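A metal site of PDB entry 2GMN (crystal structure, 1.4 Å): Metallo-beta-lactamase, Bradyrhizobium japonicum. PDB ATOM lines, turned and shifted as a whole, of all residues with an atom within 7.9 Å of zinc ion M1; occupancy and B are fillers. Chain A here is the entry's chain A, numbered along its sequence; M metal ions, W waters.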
ATOM      1  N   TRP A  14      -7.076 -11.789  16.164  1.00  0.00           N
ATOM      2  CA  TRP A  14      -7.577 -11.344  14.871  1.00  0.00           C
ATOM      3  C   TRP A  14      -8.887 -11.999  14.446  1.00  0.00           C
ATOM      4  O   TRP A  14      -9.615 -11.422  13.628  1.00  0.00           O
ATOM      5  CB  TRP A  14      -6.513 -11.557  13.792  1.00  0.00           C
ATOM      6  CG  TRP A  14      -5.386 -10.563  13.850  1.00  0.00           C
ATOM      7  CD1 TRP A  14      -5.123  -9.678  14.854  1.00  0.00           C
ATOM      8  CD2 TRP A  14      -4.363 -10.380  12.866  1.00  0.00           C
ATOM      9  NE1 TRP A  14      -3.999  -8.944  14.544  1.00  0.00           N
ATOM     10  CE2 TRP A  14      -3.514  -9.362  13.342  1.00  0.00           C
ATOM     11  CE3 TRP A  14      -4.081 -10.983  11.634  1.00  0.00           C
ATOM     12  CZ2 TRP A  14      -2.396  -8.918  12.625  1.00  0.00           C
ATOM     13  CZ3 TRP A  14      -2.955 -10.543  10.922  1.00  0.00           C
ATOM     14  CH2 TRP A  14      -2.144  -9.520  11.414  1.00  0.00           C
ATOM     15  N   THR A  80      -7.406   0.379   3.030  1.00  0.00           N
ATOM     16  CA  THR A  80      -6.277   1.102   3.616  1.00  0.00           C
ATOM     17  C   THR A  80      -4.968   0.574   3.006  1.00  0.00           C
ATOM     18  O   THR A  80      -4.178   1.328   2.454  1.00  0.00           O
ATOM     19  CB  THR A  80      -6.213   0.932   5.150  1.00  0.00           C
ATOM     20  OG1 THR A  80      -6.365  -0.455   5.479  1.00  0.00           O
ATOM     21  CG2 THR A  80      -7.283   1.762   5.836  1.00  0.00           C
ATOM     22  N   HIS A  81      -4.734  -0.733   3.099  1.00  0.00           N
ATOM     23  CA  HIS A  81      -3.534  -1.302   2.470  1.00  0.00           C
ATOM     24  C   HIS A  81      -3.721  -2.777   2.155  1.00  0.00           C
ATOM     25  O   HIS A  81      -4.530  -3.452   2.796  1.00  0.00           O
ATOM     26  CB  HIS A  81      -2.280  -1.059   3.314  1.00  0.00           C
ATOM     27  CG  HIS A  81      -2.193  -1.931   4.530  1.00  0.00           C
ATOM     28  ND1 HIS A  81      -2.684  -1.538   5.757  1.00  0.00           N
ATOM     29  CD2 HIS A  81      -1.638  -3.151   4.713  1.00  0.00           C
ATOM     30  CE1 HIS A  81      -2.454  -2.499   6.643  1.00  0.00           C
ATOM     31  NE2 HIS A  81      -1.824  -3.489   6.036  1.00  0.00           N
ATOM     32  N   ALA A  82      -2.941  -3.250   1.181  1.00  0.00           N
ATOM     33  CA  ALA A  82      -3.231  -4.519   0.544  1.00  0.00           C
ATOM     34  C   ALA A  82      -2.495  -5.705   1.176  1.00  0.00           C
ATOM     35  O   ALA A  82      -1.711  -6.363   0.488  1.00  0.00           O
ATOM     36  CB  ALA A  82      -2.914  -4.414  -0.952  1.00  0.00           C
ATOM     37  N   HIS A  83      -2.733  -5.978   2.454  1.00  0.00           N
ATOM     38  CA  HIS A  83      -2.285  -7.223   3.103  1.00  0.00           C
ATOM     39  C   HIS A  83      -3.483  -8.101   3.431  1.00  0.00           C
ATOM     40  O   HIS A  83      -4.587  -7.581   3.639  1.00  0.00           O
ATOM     41  CB  HIS A  83      -1.548  -6.939   4.397  1.00  0.00           C
ATOM     42  CG  HIS A  83      -0.211  -6.297   4.212  1.00  0.00           C
ATOM     43  ND1 HIS A  83       0.392  -5.552   5.209  1.00  0.00           N
ATOM     44  CD2 HIS A  83       0.639  -6.280   3.155  1.00  0.00           C
ATOM     45  CE1 HIS A  83       1.571  -5.119   4.768  1.00  0.00           C
ATOM     46  NE2 HIS A  83       1.731  -5.528   3.522  1.00  0.00           N
ATOM     47  N   LEU A  84      -3.268  -9.428   3.513  1.00  0.00           N
ATOM     48  CA  LEU A  84      -4.366 -10.389   3.627  1.00  0.00           C
ATOM     49  C   LEU A  84      -5.274 -10.178   4.831  1.00  0.00           C
ATOM     50  O   LEU A  84      -6.433 -10.566   4.787  1.00  0.00           O
ATOM     51  CB  LEU A  84      -3.851 -11.829   3.612  1.00  0.00           C
ATOM     52  CG  LEU A  84      -3.335 -12.448   4.910  1.00  0.00           C
ATOM     53  CD1 LEU A  84      -3.332 -13.960   4.775  1.00  0.00           C
ATOM     54  CD2 LEU A  84      -1.940 -11.919   5.289  1.00  0.00           C
ATOM     55  N   ASP A  85      -4.765  -9.553   5.891  1.00  0.00           N
ATOM     56  CA  ASP A  85      -5.598  -9.374   7.081  1.00  0.00           C
ATOM     57  C   ASP A  85      -6.614  -8.248   6.894  1.00  0.00           C
ATOM     58  O   ASP A  85      -7.489  -8.063   7.743  1.00  0.00           O
ATOM     59  CB  ASP A  85      -4.758  -9.208   8.367  1.00  0.00           C
ATOM     60  CG  ASP A  85      -3.716  -8.106   8.274  1.00  0.00           C
ATOM     61  OD1 ASP A  85      -3.039  -7.978   7.222  1.00  0.00           O
ATOM     62  OD2 ASP A  85      -3.539  -7.372   9.289  1.00  0.00           O
ATOM     63  N   HIS A  86      -6.503  -7.537   5.784  1.00  0.00           N
ATOM     64  CA  HIS A  86      -7.446  -6.459   5.428  1.00  0.00           C
ATOM     65  C   HIS A  86      -8.158  -6.677   4.099  1.00  0.00           C
ATOM     66  O   HIS A  86      -9.190  -6.069   3.845  1.00  0.00           O
ATOM     67  CB  HIS A  86      -6.745  -5.107   5.431  1.00  0.00           C
ATOM     68  CG  HIS A  86      -5.963  -4.898   6.680  1.00  0.00           C
ATOM     69  ND1 HIS A  86      -6.564  -4.725   7.911  1.00  0.00           N
ATOM     70  CD2 HIS A  86      -4.631  -4.929   6.913  1.00  0.00           C
ATOM     71  CE1 HIS A  86      -5.637  -4.632   8.842  1.00  0.00           C
ATOM     72  NE2 HIS A  86      -4.451  -4.753   8.260  1.00  0.00           N
ATOM     73  N   TYR A 116       1.926 -11.068  -0.978  1.00  0.00           N
ATOM     74  CA  TYR A 116       2.695 -10.159  -0.120  1.00  0.00           C
ATOM     75  C   TYR A 116       3.925  -9.656  -0.880  1.00  0.00           C
ATOM     76  O   TYR A 116       4.696 -10.463  -1.378  1.00  0.00           O
ATOM     77  CB  TYR A 116       3.124 -10.849   1.180  1.00  0.00           C
ATOM     78  CG  TYR A 116       3.503  -9.863   2.242  1.00  0.00           C
ATOM     79  CD1 TYR A 116       2.588  -9.456   3.191  1.00  0.00           C
ATOM     80  CD2 TYR A 116       4.782  -9.301   2.286  1.00  0.00           C
ATOM     81  CE1 TYR A 116       2.914  -8.531   4.164  1.00  0.00           C
ATOM     82  CE2 TYR A 116       5.122  -8.365   3.250  1.00  0.00           C
ATOM     83  CZ  TYR A 116       4.181  -7.975   4.183  1.00  0.00           C
ATOM     84  OH  TYR A 116       4.513  -7.034   5.142  1.00  0.00           O
ATOM     85  N   HIS A 157       4.141   1.019   5.054  1.00  0.00           N
ATOM     86  CA  HIS A 157       3.679  -0.305   5.472  1.00  0.00           C
ATOM     87  C   HIS A 157       3.306  -1.141   4.231  1.00  0.00           C
ATOM     88  O   HIS A 157       3.477  -2.363   4.200  1.00  0.00           O
ATOM     89  CB  HIS A 157       2.516  -0.177   6.449  1.00  0.00           C
ATOM     90  CG  HIS A 157       2.020  -1.494   6.955  1.00  0.00           C
ATOM     91  ND1 HIS A 157       2.588  -2.143   8.034  1.00  0.00           N
ATOM     92  CD2 HIS A 157       1.014  -2.288   6.515  1.00  0.00           C
ATOM     93  CE1 HIS A 157       1.955  -3.289   8.233  1.00  0.00           C
ATOM     94  NE2 HIS A 157       1.000  -3.404   7.321  1.00  0.00           N
ATOM     95  N   SER A 158       2.783  -0.468   3.205  1.00  0.00           N
ATOM     96  CA  SER A 158       2.629  -1.056   1.876  1.00  0.00           C
ATOM     97  C   SER A 158       2.934   0.052   0.868  1.00  0.00           C
ATOM     98  O   SER A 158       2.880   1.244   1.216  1.00  0.00           O
ATOM     99  CB  SER A 158       1.220  -1.627   1.666  1.00  0.00           C
ATOM    100  OG  SER A 158       0.302  -0.585   1.393  1.00  0.00           O
ATOM    101  N   CYS A 161      -0.291   2.199   0.502  1.00  0.00           N
ATOM    102  CA  CYS A 161      -1.015   2.467   1.749  1.00  0.00           C
ATOM    103  C   CYS A 161      -1.724   3.824   1.675  1.00  0.00           C
ATOM    104  O   CYS A 161      -1.085   4.850   1.426  1.00  0.00           O
ATOM    105  CB  CYS A 161       0.008   2.434   2.892  1.00  0.00           C
ATOM    106  SG  CYS A 161      -0.549   1.953   4.529  1.00  0.00           S
ATOM    107  N   CYS A 181      -3.752   4.289   7.569  1.00  0.00           N
ATOM    108  CA  CYS A 181      -3.595   3.040   6.824  1.00  0.00           C
ATOM    109  C   CYS A 181      -2.729   1.969   7.488  1.00  0.00           C
ATOM    110  O   CYS A 181      -2.796   0.809   7.104  1.00  0.00           O
ATOM    111  CB  CYS A 181      -3.087   3.332   5.410  1.00  0.00           C
ATOM    112  SG  CYS A 181      -1.334   3.680   5.342  1.00  0.00           S
ATOM    113  N   SER A 182      -1.918   2.387   8.446  1.00  0.00           N
ATOM    114  CA  SER A 182      -0.916   1.588   9.187  1.00  0.00           C
ATOM    115  C   SER A 182       0.477   2.142   8.913  1.00  0.00           C
ATOM    116  O   SER A 182       0.810   2.457   7.764  1.00  0.00           O
ATOM    117  CB  SER A 182      -0.910   0.093   8.878  1.00  0.00           C
ATOM    118  OG  SER A 182       0.153  -0.494   9.600  1.00  0.00           O
ATOM    119  N   GLY A 183       1.275   2.223   9.964  1.00  0.00           N
ATOM    120  CA  GLY A 183       2.677   2.631   9.854  1.00  0.00           C
ATOM    121  C   GLY A 183       3.651   1.731  10.605  1.00  0.00           C
ATOM    122  O   GLY A 183       4.775   2.143  10.933  1.00  0.00           O
ATOM    123  N   THR A 184       3.224   0.511  10.897  1.00  0.00           N
ATOM    124  CA  THR A 184       4.086  -0.444  11.586  1.00  0.00           C
ATOM    125  C   THR A 184       5.092  -1.063  10.622  1.00  0.00           C
ATOM    126  O   THR A 184       4.862  -1.108   9.407  1.00  0.00           O
ATOM    127  CB  THR A 184       3.262  -1.580  12.188  1.00  0.00           C
ATOM    128  OG1 THR A 184       2.541  -2.236  11.142  1.00  0.00           O
ATOM    129  CG2 THR A 184       2.258  -1.030  13.222  1.00  0.00           C
ATOM    130  N   VAL A 185       6.220  -1.526  11.158  1.00  0.00           N
ATOM    131  CA  VAL A 185       7.184  -2.261  10.319  1.00  0.00           C
ATOM    132  C   VAL A 185       6.690  -3.674  10.051  1.00  0.00           C
ATOM    133  O   VAL A 185       6.757  -4.154   8.905  1.00  0.00           O
ATOM    134  CB  VAL A 185       8.595  -2.270  10.940  1.00  0.00           C
ATOM    135  CG1 VAL A 185       9.564  -3.124  10.093  1.00  0.00           C
ATOM    136  CG2 VAL A 185       9.110  -0.835  11.089  1.00  0.00           C
ATOM    137  N   ALA A 186       6.208  -4.328  11.105  1.00  0.00           N
ATOM    138  CA  ALA A 186       5.618  -5.666  11.004  1.00  0.00           C
ATOM    139  C   ALA A 186       6.547  -6.621  10.237  1.00  0.00           C
ATOM    140  O   ALA A 186       7.696  -6.815  10.650  1.00  0.00           O
ATOM    141  CB  ALA A 186       4.222  -5.575  10.374  1.00  0.00           C
ATOM    142  N   LEU A 187       6.070  -7.181   9.131  1.00  0.00           N
ATOM    143  CA  LEU A 187       6.853  -8.203   8.410  1.00  0.00           C
ATOM    144  C   LEU A 187       7.804  -7.635   7.371  1.00  0.00           C
ATOM    145  O   LEU A 187       8.530  -8.394   6.732  1.00  0.00           O
ATOM    146  CB  LEU A 187       5.924  -9.216   7.731  1.00  0.00           C
ATOM    147  CG  LEU A 187       5.026 -10.051   8.633  1.00  0.00           C
ATOM    148  CD1 LEU A 187       4.188 -10.973   7.764  1.00  0.00           C
ATOM    149  CD2 LEU A 187       5.801 -10.844   9.675  1.00  0.00           C
ATOM    150  N   ASN A 188       7.795  -6.321   7.191  1.00  0.00           N
ATOM    151  CA  ASN A 188       8.533  -5.704   6.085  1.00  0.00           C
ATOM    152  C   ASN A 188      10.042  -5.712   6.307  1.00  0.00           C
ATOM    153  O   ASN A 188      10.509  -5.554   7.431  1.00  0.00           O
ATOM    154  CB  ASN A 188       8.062  -4.262   5.862  1.00  0.00           C
ATOM    155  CG  ASN A 188       6.681  -4.197   5.246  1.00  0.00           C
ATOM    156  OD1 ASN A 188       6.267  -5.115   4.522  1.00  0.00           O
ATOM    157  ND2 ASN A 188       5.952  -3.111   5.512  1.00  0.00           N
ATOM    158  N   PRO A 221      -6.557   0.231  10.860  1.00  0.00           N
ATOM    159  CA  PRO A 221      -6.984  -1.114  10.449  1.00  0.00           C
ATOM    160  C   PRO A 221      -6.860  -2.210  11.511  1.00  0.00           C
ATOM    161  O   PRO A 221      -7.302  -3.346  11.288  1.00  0.00           O
ATOM    162  CB  PRO A 221      -6.097  -1.399   9.232  1.00  0.00           C
ATOM    163  CG  PRO A 221      -4.924  -0.486   9.348  1.00  0.00           C
ATOM    164  CD  PRO A 221      -5.217   0.577  10.360  1.00  0.00           C
ATOM    165  N   HIS A 222      -6.289  -1.869  12.666  1.00  0.00           N
ATOM    166  CA  HIS A 222      -6.315  -2.720  13.845  1.00  0.00           C
ATOM    167  C   HIS A 222      -6.744  -1.855  15.021  1.00  0.00           C
ATOM    168  O   HIS A 222      -6.344  -0.695  15.099  1.00  0.00           O
ATOM    169  CB  HIS A 222      -4.915  -3.307  14.091  1.00  0.00           C
ATOM    170  CG  HIS A 222      -4.466  -4.241  13.016  1.00  0.00           C
ATOM    171  ND1 HIS A 222      -4.861  -5.570  12.979  1.00  0.00           N
ATOM    172  CD2 HIS A 222      -3.657  -4.059  11.944  1.00  0.00           C
ATOM    173  CE1 HIS A 222      -4.322  -6.152  11.921  1.00  0.00           C
ATOM    174  NE2 HIS A 222      -3.588  -5.259  11.279  1.00  0.00           N
HETATM  175 ZN    ZN M   1      -0.458  -4.777   6.952  1.00  0.00          ZN
HETATM  176 ZN    ZN M   2      -2.820  -5.458   9.372  1.00  0.00          ZN
HETATM  177  O   HOH W   1      -1.321  -6.120   8.097  1.00  0.00           O
HETATM  178  O   HOH W   2       1.100  -6.582   9.086  1.00  0.00           O
HETATM  179  O   HOH W   3      -1.481  -3.325   9.700  1.00  0.00           O
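Of the 22 residues printed, 3 come within 4 Å of zinc ion M1.
The nearest printed residue that does not touch zinc ion M1 is Asp 85 (4.1 Å).
Zinc ion M1 is bound by water W1 (2.0 Å).
Zinc ion M1 is bound by NE2 of His 157, at 2.0 Å.
ND1 of His 83 binds zinc ion M1, at 2.1 Å.
NE2 of His 81 is bound to zinc ion M1 (2.1 Å).
The side-chain hydroxyl (OG) of Ser 182 lies within hydrogen-bond range of a ring nitrogen (ND1) of His 157, 3.3 Å away.
A ring nitrogen (ND1) of His 157 sits at hydrogen-bond distance from the backbone carbonyl oxygen (O) of Thr 184 (2.9 Å).
O of His 157 lies within hydrogen-bond range of ND2 of Asn 188 (2.9 Å).
ND1 of His 81 sits at hydrogen-bond distance from O of Cys 181 (2.7 Å).
The side-chain sulfur (SG) of Cys 161 is disulfide-bonded to the side-chain sulfur (SG) of Cys 181, at 2.1 Å.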
